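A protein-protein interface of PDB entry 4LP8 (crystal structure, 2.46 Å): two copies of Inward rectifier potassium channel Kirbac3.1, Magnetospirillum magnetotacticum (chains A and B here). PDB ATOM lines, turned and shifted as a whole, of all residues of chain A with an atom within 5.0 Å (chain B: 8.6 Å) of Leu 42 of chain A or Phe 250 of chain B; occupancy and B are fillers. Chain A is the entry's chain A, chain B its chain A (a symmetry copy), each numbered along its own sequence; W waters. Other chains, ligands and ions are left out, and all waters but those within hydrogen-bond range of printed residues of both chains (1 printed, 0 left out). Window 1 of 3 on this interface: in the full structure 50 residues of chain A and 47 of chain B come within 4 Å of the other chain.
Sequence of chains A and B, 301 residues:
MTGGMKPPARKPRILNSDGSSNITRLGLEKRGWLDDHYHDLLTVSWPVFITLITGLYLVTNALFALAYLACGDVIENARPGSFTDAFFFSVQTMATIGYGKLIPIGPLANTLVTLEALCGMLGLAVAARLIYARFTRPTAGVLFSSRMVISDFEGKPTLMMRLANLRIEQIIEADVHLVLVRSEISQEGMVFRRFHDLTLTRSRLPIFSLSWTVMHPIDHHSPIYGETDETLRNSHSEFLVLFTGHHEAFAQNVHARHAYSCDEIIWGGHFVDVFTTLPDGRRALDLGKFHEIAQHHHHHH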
ATOM      1  N   ASP A  36      18.692   3.688 -21.736  1.00  0.00           N
ATOM      2  CA  ASP A  36      18.457   5.081 -21.317  1.00  0.00           C
ATOM      3  C   ASP A  36      19.429   5.395 -20.145  1.00  0.00           C
ATOM      4  O   ASP A  36      19.033   5.884 -19.090  1.00  0.00           O
ATOM      5  CB  ASP A  36      16.969   5.211 -20.926  1.00  0.00           C
ATOM      6  CG  ASP A  36      16.374   6.596 -20.872  1.00  0.00           C
ATOM      7  OD1 ASP A  36      16.826   7.476 -21.656  1.00  0.00           O
ATOM      8  OD2 ASP A  36      15.396   6.787 -20.110  1.00  0.00           O
ATOM      9  N   TYR A  38      21.955   7.568 -19.446  1.00  0.00           N
ATOM     10  CA  TYR A  38      22.167   8.913 -18.935  1.00  0.00           C
ATOM     11  C   TYR A  38      20.997   9.386 -18.055  1.00  0.00           C
ATOM     12  O   TYR A  38      21.253   9.903 -16.966  1.00  0.00           O
ATOM     13  CB  TYR A  38      22.457   9.886 -20.088  1.00  0.00           C
ATOM     14  CG  TYR A  38      22.681  11.308 -19.643  1.00  0.00           C
ATOM     15  CD1 TYR A  38      23.463  11.599 -18.523  1.00  0.00           C
ATOM     16  CD2 TYR A  38      22.067  12.366 -20.300  1.00  0.00           C
ATOM     17  CE1 TYR A  38      23.599  12.905 -18.059  1.00  0.00           C
ATOM     18  CE2 TYR A  38      22.244  13.685 -19.874  1.00  0.00           C
ATOM     19  CZ  TYR A  38      23.016  13.948 -18.763  1.00  0.00           C
ATOM     20  OH  TYR A  38      23.160  15.246 -18.354  1.00  0.00           O
ATOM     21  N   HIS A  39      19.741   9.211 -18.507  1.00  0.00           N
ATOM     22  CA  HIS A  39      18.547   9.551 -17.738  1.00  0.00           C
ATOM     23  C   HIS A  39      18.540   8.779 -16.421  1.00  0.00           C
ATOM     24  O   HIS A  39      18.370   9.384 -15.362  1.00  0.00           O
ATOM     25  CB  HIS A  39      17.294   9.209 -18.557  1.00  0.00           C
ATOM     26  CG  HIS A  39      16.035   9.117 -17.748  1.00  0.00           C
ATOM     27  ND1 HIS A  39      15.676   7.953 -17.110  1.00  0.00           N
ATOM     28  CD2 HIS A  39      15.090  10.052 -17.510  1.00  0.00           C
ATOM     29  CE1 HIS A  39      14.550   8.223 -16.481  1.00  0.00           C
ATOM     30  NE2 HIS A  39      14.154   9.468 -16.702  1.00  0.00           N
ATOM     31  N   ASP A  40      18.753   7.441 -16.490  1.00  0.00           N
ATOM     32  CA  ASP A  40      18.744   6.564 -15.336  1.00  0.00           C
ATOM     33  C   ASP A  40      19.860   6.904 -14.381  1.00  0.00           C
ATOM     34  O   ASP A  40      19.666   6.763 -13.173  1.00  0.00           O
ATOM     35  CB  ASP A  40      18.823   5.077 -15.753  1.00  0.00           C
ATOM     36  CG  ASP A  40      17.647   4.557 -16.583  1.00  0.00           C
ATOM     37  OD1 ASP A  40      16.569   5.195 -16.569  1.00  0.00           O
ATOM     38  OD2 ASP A  40      17.807   3.524 -17.246  1.00  0.00           O
ATOM     39  N   LEU A  41      21.022   7.374 -14.887  1.00  0.00           N
ATOM     40  CA  LEU A  41      22.128   7.747 -13.997  1.00  0.00           C
ATOM     41  C   LEU A  41      21.810   9.037 -13.232  1.00  0.00           C
ATOM     42  O   LEU A  41      22.330   9.225 -12.142  1.00  0.00           O
ATOM     43  CB  LEU A  41      23.467   7.867 -14.736  1.00  0.00           C
ATOM     44  CG  LEU A  41      24.148   6.538 -15.055  1.00  0.00           C
ATOM     45  CD1 LEU A  41      25.133   6.679 -16.214  1.00  0.00           C
ATOM     46  CD2 LEU A  41      24.770   5.906 -13.811  1.00  0.00           C
ATOM     47  N   LEU A  42      20.913   9.880 -13.763  1.00  0.00           N
ATOM     48  CA  LEU A  42      20.521  11.133 -13.132  1.00  0.00           C
ATOM     49  C   LEU A  42      19.315  11.005 -12.208  1.00  0.00           C
ATOM     50  O   LEU A  42      19.258  11.713 -11.199  1.00  0.00           O
ATOM     51  CB  LEU A  42      20.198  12.187 -14.184  1.00  0.00           C
ATOM     52  CG  LEU A  42      21.342  12.694 -15.039  1.00  0.00           C
ATOM     53  CD1 LEU A  42      20.795  13.627 -16.127  1.00  0.00           C
ATOM     54  CD2 LEU A  42      22.406  13.384 -14.183  1.00  0.00           C
ATOM     55  N   THR A  43      18.340  10.140 -12.565  1.00  0.00           N
ATOM     56  CA  THR A  43      17.080  10.021 -11.838  1.00  0.00           C
ATOM     57  C   THR A  43      17.060   8.897 -10.774  1.00  0.00           C
ATOM     58  O   THR A  43      16.177   8.884  -9.908  1.00  0.00           O
ATOM     59  CB  THR A  43      15.930   9.870 -12.845  1.00  0.00           C
ATOM     60  OG1 THR A  43      16.122   8.685 -13.616  1.00  0.00           O
ATOM     61  CG2 THR A  43      15.826  11.061 -13.753  1.00  0.00           C
ATOM     62  N   VAL A  44      18.014   7.979 -10.834  1.00  0.00           N
ATOM     63  CA  VAL A  44      18.153   6.873  -9.881  1.00  0.00           C
ATOM     64  C   VAL A  44      18.511   7.436  -8.473  1.00  0.00           C
ATOM     65  O   VAL A  44      19.109   8.508  -8.386  1.00  0.00           O
ATOM     66  CB  VAL A  44      19.186   5.892 -10.472  1.00  0.00           C
ATOM     67  CG1 VAL A  44      20.560   5.944  -9.807  1.00  0.00           C
ATOM     68  CG2 VAL A  44      18.626   4.497 -10.586  1.00  0.00           C
ATOM     69  N   LEU A 130      29.410  13.200 -13.224  1.00  0.00           N
ATOM     70  CA  LEU A 130      28.063  12.682 -13.078  1.00  0.00           C
ATOM     71  C   LEU A 130      27.557  12.961 -11.652  1.00  0.00           C
ATOM     72  O   LEU A 130      26.404  13.334 -11.495  1.00  0.00           O
ATOM     73  CB  LEU A 130      28.162  11.171 -13.347  1.00  0.00           C
ATOM     74  CG  LEU A 130      27.123  10.412 -14.151  1.00  0.00           C
ATOM     75  CD1 LEU A 130      26.770  11.114 -15.477  1.00  0.00           C
ATOM     76  CD2 LEU A 130      27.657   9.027 -14.458  1.00  0.00           C
ATOM     77  N   ALA A 133      26.771  16.654 -11.568  1.00  0.00           N
ATOM     78  CA  ALA A 133      25.526  16.925 -12.288  1.00  0.00           C
ATOM     79  C   ALA A 133      24.317  16.607 -11.406  1.00  0.00           C
ATOM     80  O   ALA A 133      23.349  17.364 -11.380  1.00  0.00           O
ATOM     81  CB  ALA A 133      25.467  16.108 -13.568  1.00  0.00           C
ATOM     82  N   ARG A 134      24.362  15.490 -10.694  1.00  0.00           N
ATOM     83  CA  ARG A 134      23.274  15.092  -9.811  1.00  0.00           C
ATOM     84  C   ARG A 134      23.134  16.024  -8.615  1.00  0.00           C
ATOM     85  O   ARG A 134      22.050  16.143  -8.062  1.00  0.00           O
ATOM     86  CB  ARG A 134      23.526  13.685  -9.290  1.00  0.00           C
ATOM     87  CG  ARG A 134      23.338  12.577 -10.309  1.00  0.00           C
ATOM     88  CD  ARG A 134      23.672  11.267  -9.652  1.00  0.00           C
ATOM     89  NE  ARG A 134      22.789  11.013  -8.518  1.00  0.00           N
ATOM     90  CZ  ARG A 134      21.652  10.341  -8.607  1.00  0.00           C
ATOM     91  NH1 ARG A 134      21.264   9.832  -9.771  1.00  0.00           N
ATOM     92  NH2 ARG A 134      20.897  10.160  -7.534  1.00  0.00           N
ATOM     93  N   ARG A 137      21.664  20.515  -9.185  1.00  0.00           N
ATOM     94  CA  ARG A 137      20.340  20.809  -9.727  1.00  0.00           C
ATOM     95  C   ARG A 137      19.797  22.035  -9.012  1.00  0.00           C
ATOM     96  O   ARG A 137      19.674  21.990  -7.776  1.00  0.00           O
ATOM     97  CB  ARG A 137      19.394  19.624  -9.534  1.00  0.00           C
ATOM     98  CG  ARG A 137      19.498  18.563 -10.601  1.00  0.00           C
ATOM     99  CD  ARG A 137      18.526  17.448 -10.300  1.00  0.00           C
ATOM    100  NE  ARG A 137      18.777  16.285 -11.144  1.00  0.00           N
ATOM    101  CZ  ARG A 137      18.086  15.994 -12.237  1.00  0.00           C
ATOM    102  NH1 ARG A 137      18.383  14.916 -12.945  1.00  0.00           N
ATOM    103  NH2 ARG A 137      17.089  16.775 -12.628  1.00  0.00           N
ATOM    104  N   TYR B 132      32.625  12.642 -21.393  1.00  0.00           N
ATOM    105  CA  TYR B 132      31.421  13.056 -20.680  1.00  0.00           C
ATOM    106  C   TYR B 132      30.444  13.799 -21.618  1.00  0.00           C
ATOM    107  O   TYR B 132      29.238  13.568 -21.522  1.00  0.00           O
ATOM    108  CB  TYR B 132      31.762  13.947 -19.457  1.00  0.00           C
ATOM    109  CG  TYR B 132      30.538  14.267 -18.624  1.00  0.00           C
ATOM    110  CD1 TYR B 132      30.129  13.422 -17.600  1.00  0.00           C
ATOM    111  CD2 TYR B 132      29.772  15.411 -18.875  1.00  0.00           C
ATOM    112  CE1 TYR B 132      28.986  13.695 -16.850  1.00  0.00           C
ATOM    113  CE2 TYR B 132      28.632  15.702 -18.125  1.00  0.00           C
ATOM    114  CZ  TYR B 132      28.234  14.829 -17.122  1.00  0.00           C
ATOM    115  OH  TYR B 132      27.099  15.085 -16.389  1.00  0.00           O
ATOM    116  N   PHE B 135      28.760  11.473 -23.988  1.00  0.00           N
ATOM    117  CA  PHE B 135      27.966  10.511 -23.220  1.00  0.00           C
ATOM    118  C   PHE B 135      26.696  11.093 -22.651  1.00  0.00           C
ATOM    119  O   PHE B 135      25.767  10.336 -22.386  1.00  0.00           O
ATOM    120  CB  PHE B 135      28.853   9.987 -22.067  1.00  0.00           C
ATOM    121  CG  PHE B 135      28.391   8.838 -21.205  1.00  0.00           C
ATOM    122  CD1 PHE B 135      28.441   7.527 -21.678  1.00  0.00           C
ATOM    123  CD2 PHE B 135      28.053   9.042 -19.866  1.00  0.00           C
ATOM    124  CE1 PHE B 135      28.089   6.449 -20.851  1.00  0.00           C
ATOM    125  CE2 PHE B 135      27.684   7.963 -19.045  1.00  0.00           C
ATOM    126  CZ  PHE B 135      27.717   6.673 -19.541  1.00  0.00           C
ATOM    127  N   THR B 136      26.637  12.413 -22.455  1.00  0.00           N
ATOM    128  CA  THR B 136      25.526  13.044 -21.760  1.00  0.00           C
ATOM    129  C   THR B 136      24.598  13.842 -22.661  1.00  0.00           C
ATOM    130  O   THR B 136      24.043  14.866 -22.226  1.00  0.00           O
ATOM    131  CB  THR B 136      26.056  13.869 -20.610  1.00  0.00           C
ATOM    132  OG1 THR B 136      27.007  14.826 -21.102  1.00  0.00           O
ATOM    133  CG2 THR B 136      26.685  12.995 -19.538  1.00  0.00           C
ATOM    134  N   ARG B 137      24.420  13.359 -23.918  1.00  0.00           N
ATOM    135  CA  ARG B 137      23.497  13.957 -24.880  1.00  0.00           C
ATOM    136  C   ARG B 137      22.082  13.565 -24.487  1.00  0.00           C
ATOM    137  O   ARG B 137      21.801  12.355 -24.427  1.00  0.00           O
ATOM    138  CB  ARG B 137      23.802  13.478 -26.300  1.00  0.00           C
ATOM    139  CG  ARG B 137      24.892  14.252 -26.998  1.00  0.00           C
ATOM    140  CD  ARG B 137      25.105  13.685 -28.381  1.00  0.00           C
ATOM    141  NE  ARG B 137      26.319  14.218 -28.990  1.00  0.00           N
ATOM    142  CZ  ARG B 137      26.339  15.205 -29.874  1.00  0.00           C
ATOM    143  NH1 ARG B 137      27.489  15.627 -30.375  1.00  0.00           N
ATOM    144  NH2 ARG B 137      25.209  15.776 -30.268  1.00  0.00           N
ATOM    145  N   PRO B 138      21.162  14.524 -24.130  1.00  0.00           N
ATOM    146  CA  PRO B 138      19.807  14.084 -23.729  1.00  0.00           C
ATOM    147  C   PRO B 138      18.882  13.811 -24.897  1.00  0.00           C
ATOM    148  O   PRO B 138      18.905  14.517 -25.908  1.00  0.00           O
ATOM    149  CB  PRO B 138      19.267  15.254 -22.903  1.00  0.00           C
ATOM    150  CG  PRO B 138      20.012  16.437 -23.374  1.00  0.00           C
ATOM    151  CD  PRO B 138      21.264  16.002 -24.091  1.00  0.00           C
ATOM    152  N   THR B 139      18.053  12.794 -24.749  1.00  0.00           N
ATOM    153  CA  THR B 139      17.055  12.455 -25.759  1.00  0.00           C
ATOM    154  C   THR B 139      15.693  12.854 -25.201  1.00  0.00           C
ATOM    155  O   THR B 139      15.428  12.683 -23.992  1.00  0.00           O
ATOM    156  CB  THR B 139      17.149  11.008 -26.141  1.00  0.00           C
ATOM    157  OG1 THR B 139      16.758  10.227 -25.019  1.00  0.00           O
ATOM    158  CG2 THR B 139      18.533  10.629 -26.608  1.00  0.00           C
ATOM    159  N   ALA B 140      14.845  13.418 -26.070  1.00  0.00           N
ATOM    160  CA  ALA B 140      13.535  13.943 -25.683  1.00  0.00           C
ATOM    161  C   ALA B 140      12.589  12.849 -25.162  1.00  0.00           C
ATOM    162  O   ALA B 140      11.813  13.119 -24.244  1.00  0.00           O
ATOM    163  CB  ALA B 140      12.907  14.703 -26.841  1.00  0.00           C
ATOM    164  N   GLY B 141      12.732  11.625 -25.660  1.00  0.00           N
ATOM    165  CA  GLY B 141      11.905  10.489 -25.258  1.00  0.00           C
ATOM    166  C   GLY B 141      10.452  10.759 -25.574  1.00  0.00           C
ATOM    167  O   GLY B 141       9.578  10.554 -24.725  1.00  0.00           O
ATOM    168  N   ASN B 165       4.867  11.701 -24.066  1.00  0.00           N
ATOM    169  CA  ASN B 165       6.076  11.693 -23.254  1.00  0.00           C
ATOM    170  C   ASN B 165       6.321  10.227 -22.846  1.00  0.00           C
ATOM    171  O   ASN B 165       5.464   9.644 -22.191  1.00  0.00           O
ATOM    172  CB  ASN B 165       5.920  12.629 -22.040  1.00  0.00           C
ATOM    173  CG  ASN B 165       7.189  12.856 -21.259  1.00  0.00           C
ATOM    174  OD1 ASN B 165       8.183  12.110 -21.350  1.00  0.00           O
ATOM    175  ND2 ASN B 165       7.168  13.861 -20.424  1.00  0.00           N
ATOM    176  N   ARG B 167       8.563   9.095 -20.874  1.00  0.00           N
ATOM    177  CA  ARG B 167       9.143   9.027 -19.544  1.00  0.00           C
ATOM    178  C   ARG B 167       8.220   9.626 -18.473  1.00  0.00           C
ATOM    179  O   ARG B 167       7.268  10.359 -18.766  1.00  0.00           O
ATOM    180  CB  ARG B 167      10.504   9.745 -19.530  1.00  0.00           C
ATOM    181  CG  ARG B 167      11.528   9.128 -20.465  1.00  0.00           C
ATOM    182  CD  ARG B 167      12.865   9.642 -20.042  1.00  0.00           C
ATOM    183  NE  ARG B 167      13.947   9.297 -20.954  1.00  0.00           N
ATOM    184  CZ  ARG B 167      14.342  10.060 -21.957  1.00  0.00           C
ATOM    185  NH1 ARG B 167      13.684  11.174 -22.251  1.00  0.00           N
ATOM    186  NH2 ARG B 167      15.384   9.707 -22.693  1.00  0.00           N
ATOM    187  N   GLU B 169       9.159  11.747 -16.111  1.00  0.00           N
ATOM    188  CA  GLU B 169       9.506  13.144 -15.847  1.00  0.00           C
ATOM    189  C   GLU B 169       8.923  14.034 -16.915  1.00  0.00           C
ATOM    190  O   GLU B 169       8.814  13.656 -18.089  1.00  0.00           O
ATOM    191  CB  GLU B 169      11.023  13.356 -15.722  1.00  0.00           C
ATOM    192  CG  GLU B 169      11.677  12.529 -14.623  1.00  0.00           C
ATOM    193  CD  GLU B 169      12.039  11.112 -15.031  1.00  0.00           C
ATOM    194  OE1 GLU B 169      11.882  10.769 -16.228  1.00  0.00           O
ATOM    195  OE2 GLU B 169      12.451  10.330 -14.142  1.00  0.00           O
ATOM    196  N   GLN B 170       8.508  15.219 -16.485  1.00  0.00           N
ATOM    197  CA  GLN B 170       7.822  16.190 -17.331  1.00  0.00           C
ATOM    198  C   GLN B 170       8.742  17.032 -18.198  1.00  0.00           C
ATOM    199  O   GLN B 170       9.904  17.271 -17.868  1.00  0.00           O
ATOM    200  CB  GLN B 170       6.985  17.112 -16.439  1.00  0.00           C
ATOM    201  CG  GLN B 170       5.579  16.587 -16.270  1.00  0.00           C
ATOM    202  CD  GLN B 170       5.160  16.527 -14.838  1.00  0.00           C
ATOM    203  OE1 GLN B 170       5.205  17.521 -14.111  1.00  0.00           O
ATOM    204  NE2 GLN B 170       4.682  15.369 -14.424  1.00  0.00           N
ATOM    205  N   ILE B 171       8.180  17.507 -19.301  1.00  0.00           N
ATOM    206  CA  ILE B 171       8.812  18.455 -20.209  1.00  0.00           C
ATOM    207  C   ILE B 171       8.030  19.744 -20.004  1.00  0.00           C
ATOM    208  O   ILE B 171       6.802  19.760 -20.089  1.00  0.00           O
ATOM    209  CB  ILE B 171       8.878  17.982 -21.703  1.00  0.00           C
ATOM    210  CG1 ILE B 171       9.642  16.637 -21.835  1.00  0.00           C
ATOM    211  CG2 ILE B 171       9.484  19.078 -22.622  1.00  0.00           C
ATOM    212  CD1 ILE B 171       9.276  15.784 -23.020  1.00  0.00           C
ATOM    213  N   GLY B 245      11.523  21.388 -25.894  1.00  0.00           N
ATOM    214  CA  GLY B 245      11.084  21.503 -24.513  1.00  0.00           C
ATOM    215  C   GLY B 245      12.237  21.404 -23.548  1.00  0.00           C
ATOM    216  O   GLY B 245      13.350  21.047 -23.942  1.00  0.00           O
ATOM    217  N   HIS B 246      11.988  21.753 -22.279  1.00  0.00           N
ATOM    218  CA  HIS B 246      12.971  21.614 -21.212  1.00  0.00           C
ATOM    219  C   HIS B 246      12.625  20.348 -20.453  1.00  0.00           C
ATOM    220  O   HIS B 246      11.505  20.236 -19.979  1.00  0.00           O
ATOM    221  CB  HIS B 246      12.931  22.847 -20.305  1.00  0.00           C
ATOM    222  CG  HIS B 246      13.943  22.794 -19.209  1.00  0.00           C
ATOM    223  ND1 HIS B 246      15.253  23.190 -19.421  1.00  0.00           N
ATOM    224  CD2 HIS B 246      13.811  22.366 -17.935  1.00  0.00           C
ATOM    225  CE1 HIS B 246      15.879  22.974 -18.275  1.00  0.00           C
ATOM    226  NE2 HIS B 246      15.046  22.501 -17.344  1.00  0.00           N
ATOM    227  N   HIS B 247      13.532  19.383 -20.372  1.00  0.00           N
ATOM    228  CA  HIS B 247      13.261  18.122 -19.698  1.00  0.00           C
ATOM    229  C   HIS B 247      13.722  18.168 -18.285  1.00  0.00           C
ATOM    230  O   HIS B 247      14.907  18.392 -18.028  1.00  0.00           O
ATOM    231  CB  HIS B 247      13.933  16.950 -20.421  1.00  0.00           C
ATOM    232  CG  HIS B 247      13.191  15.651 -20.270  1.00  0.00           C
ATOM    233  ND1 HIS B 247      12.929  15.102 -19.020  1.00  0.00           N
ATOM    234  CD2 HIS B 247      12.669  14.841 -21.216  1.00  0.00           C
ATOM    235  CE1 HIS B 247      12.256  13.987 -19.253  1.00  0.00           C
ATOM    236  NE2 HIS B 247      12.097  13.779 -20.559  1.00  0.00           N
ATOM    237  N   GLU B 248      12.795  17.902 -17.354  1.00  0.00           N
ATOM    238  CA  GLU B 248      13.063  17.889 -15.916  1.00  0.00           C
ATOM    239  C   GLU B 248      14.053  16.810 -15.487  1.00  0.00           C
ATOM    240  O   GLU B 248      14.817  17.058 -14.556  1.00  0.00           O
ATOM    241  CB  GLU B 248      11.767  17.730 -15.138  1.00  0.00           C
ATOM    242  CG  GLU B 248      10.976  19.024 -15.138  1.00  0.00           C
ATOM    243  CD  GLU B 248       9.854  19.090 -14.134  1.00  0.00           C
ATOM    244  OE1 GLU B 248       9.609  18.075 -13.446  1.00  0.00           O
ATOM    245  OE2 GLU B 248       9.225  20.164 -14.022  1.00  0.00           O
ATOM    246  N   ALA B 249      14.059  15.628 -16.139  1.00  0.00           N
ATOM    247  CA  ALA B 249      15.009  14.548 -15.781  1.00  0.00           C
ATOM    248  C   ALA B 249      16.451  14.977 -16.041  1.00  0.00           C
ATOM    249  O   ALA B 249      17.320  14.687 -15.247  1.00  0.00           O
ATOM    250  CB  ALA B 249      14.702  13.287 -16.575  1.00  0.00           C
ATOM    251  N   PHE B 250      16.694  15.682 -17.154  1.00  0.00           N
ATOM    252  CA  PHE B 250      18.014  16.129 -17.546  1.00  0.00           C
ATOM    253  C   PHE B 250      18.341  17.541 -17.047  1.00  0.00           C
ATOM    254  O   PHE B 250      19.512  17.901 -17.051  1.00  0.00           O
ATOM    255  CB  PHE B 250      18.153  16.072 -19.095  1.00  0.00           C
ATOM    256  CG  PHE B 250      17.888  14.697 -19.682  1.00  0.00           C
ATOM    257  CD1 PHE B 250      18.829  13.675 -19.566  1.00  0.00           C
ATOM    258  CD2 PHE B 250      16.695  14.419 -20.335  1.00  0.00           C
ATOM    259  CE1 PHE B 250      18.580  12.402 -20.088  1.00  0.00           C
ATOM    260  CE2 PHE B 250      16.443  13.135 -20.846  1.00  0.00           C
ATOM    261  CZ  PHE B 250      17.391  12.138 -20.717  1.00  0.00           C
ATOM    262  N   ALA B 251      17.327  18.358 -16.664  1.00  0.00           N
ATOM    263  CA  ALA B 251      17.502  19.779 -16.314  1.00  0.00           C
ATOM    264  C   ALA B 251      18.268  20.438 -17.490  1.00  0.00           C
ATOM    265  O   ALA B 251      19.245  21.172 -17.315  1.00  0.00           O
ATOM    266  CB  ALA B 251      18.226  19.948 -14.979  1.00  0.00           C
ATOM    267  N   GLN B 252      17.858  20.035 -18.704  1.00  0.00           N
ATOM    268  CA  GLN B 252      18.367  20.481 -20.004  1.00  0.00           C
ATOM    269  C   GLN B 252      17.250  20.531 -21.014  1.00  0.00           C
ATOM    270  O   GLN B 252      16.310  19.725 -20.938  1.00  0.00           O
ATOM    271  CB  GLN B 252      19.446  19.529 -20.561  1.00  0.00           C
ATOM    272  CG  GLN B 252      20.785  19.576 -19.876  1.00  0.00           C
ATOM    273  CD  GLN B 252      21.635  18.432 -20.360  1.00  0.00           C
ATOM    274  OE1 GLN B 252      22.266  18.513 -21.418  1.00  0.00           O
ATOM    275  NE2 GLN B 252      21.609  17.321 -19.627  1.00  0.00           N
ATOM    276  N   ASN B 253      17.438  21.356 -22.046  1.00  0.00           N
ATOM    277  CA  ASN B 253      16.522  21.419 -23.175  1.00  0.00           C
ATOM    278  C   ASN B 253      16.713  20.203 -24.055  1.00  0.00           C
ATOM    279  O   ASN B 253      17.802  19.620 -24.102  1.00  0.00           O
ATOM    280  CB  ASN B 253      16.707  22.689 -23.975  1.00  0.00           C
ATOM    281  CG  ASN B 253      16.197  23.911 -23.270  1.00  0.00           C
ATOM    282  OD1 ASN B 253      15.588  23.853 -22.204  1.00  0.00           O
ATOM    283  ND2 ASN B 253      16.453  25.050 -23.849  1.00  0.00           N
ATOM    284  N   VAL B 254      15.623  19.794 -24.697  1.00  0.00           N
ATOM    285  CA  VAL B 254      15.521  18.654 -25.599  1.00  0.00           C
ATOM    286  C   VAL B 254      14.704  19.037 -26.822  1.00  0.00           C
ATOM    287  O   VAL B 254      13.913  19.975 -26.765  1.00  0.00           O
ATOM    288  CB  VAL B 254      14.918  17.386 -24.928  1.00  0.00           C
ATOM    289  CG1 VAL B 254      15.897  16.762 -23.930  1.00  0.00           C
ATOM    290  CG2 VAL B 254      13.541  17.656 -24.307  1.00  0.00           C
HETATM  291  O   HOH W   1      25.275  16.696 -17.465  1.00  0.00           O
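Among the printed residues, merely in contact across the chains: Tyr 38 of chain A with Thr 136 of chain B, Tyr 38 of chain A with Phe 250 of chain B, His 39 of chain A with Arg 167 of chain B, His 39 of chain A with Ala 249 of chain B, His 39 of chain A with Phe 250 of chain B, Leu 42 of chain A with Ala 249 of chain B, Leu 42 of chain A with Phe 250 of chain B, Thr 43 of chain A with Glu 169 of chain B, Thr 43 of chain A with Ala 249 of chain B, Leu 130 of chain A with Tyr 132 of chain B and Ala 133 of chain A with Tyr 132 of chain B.
OH of Tyr 38 of chain A lies within hydrogen-bond range of NE2 of Gln 252 of chain B, 2.9 Å away.
The guanidinium group of Arg 137 of chain A sits at hydrogen-bond distance from the backbone carbonyl oxygen of Glu 248 of chain B (3.0 Å).
OD1 of Asp 36 of chain A is in salt-bridge range of NH2 of Arg 167 of chain B.
A ring nitrogen (NE2) of His 39 of chain A is in hydrogen-bond range of the side-chain carboxylate (OE1) of Glu 169 of chain B (2.7 Å).
The backbone carbonyl oxygen (O) of Ala 249 of chain B lies within hydrogen-bond range of the guanidinium group (NH1) of Arg 137 of chain A (2.5 Å).
Water W1 lies within hydrogen-bond range of the side-chain hydroxyl (OH) of Tyr 132 of chain B (2.7 Å) and the side-chain hydroxyl (OH) of Tyr 38 of chain A (2.7 Å).
Of chain B, only Ala 249 (3.7 Å) and Phe 250 (3.96 Å) come within 4 Å of Leu 42 of chain A.
Of the printed residues of chain B, Thr 43 of chain A touches Glu 169 and Ala 249.
Printed residues of chain A within 4 Å of Tyr 132 of chain B: Leu 130 (3.7 Å) and Ala 133 (3.4 Å).
Of the printed residues of chain A, Thr 136 of chain B touches Tyr 38.
Of the printed residues of chain A, Arg 167 of chain B touches Asp 36 (2.9 Å) and His 39 (3.4 Å).
Printed residues of chain A within 4 Å of Glu 248 of chain B: Arg 137 (3.0 Å).
Of the printed residues of chain A, Phe 250 of chain B touches Tyr 38, His 39 and Leu 42.
The nearest residue of chain B that does not touch Leu 42 of chain A is Gln 252 of chain B (5.2 Å).
The nearest printed residue of chain A that does not touch Phe 250 of chain B is Arg 137 of chain A (4.6 Å).
Of the 23 printed residues of chain B, 8 touch a printed residue of chain A.
Of the 12 printed residues of chain A, 8 touch a printed residue of chain B.
Hydrophobic or aromatic side chains of chain A within 4 Å of the printed part of chain B: Tyr 38, His 39, Leu 42, Leu 130 and Ala 133.
Among the printed residues, 16 pairs touch across the chains.
O of His 39 of chain A lies within hydrogen-bond range of OG1 of Thr 43 of chain A (2.9 Å).
O of Glu 169 of chain B sits at hydrogen-bond distance from ND2 of Asn 165 of chain B (2.9 Å).
The side-chain amide oxygen (OD1) of Asn 165 of chain B is in hydrogen-bond range of the backbone NH (N) of Arg 167 of chain B, at 3.1 Å.
The guanidinium group of Arg 167 of chain B is in hydrogen-bond range of a ring nitrogen (NE2) of His 247 of chain B (3.5 Å).
The side-chain carboxylate (OD1) of Asp 40 of chain A is in hydrogen-bond range of a ring nitrogen (ND1) of His 39 of chain A.
A ring nitrogen (ND1) of His 39 of chain A lies within hydrogen-bond range of the side-chain carboxylate of Asp 36 of chain A, 3.2 Å away.
Position printed for both chains: 137.
Of the 16 pairs that touch across the chains among the printed residues, none has its exchanged pair printed and touching as well.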
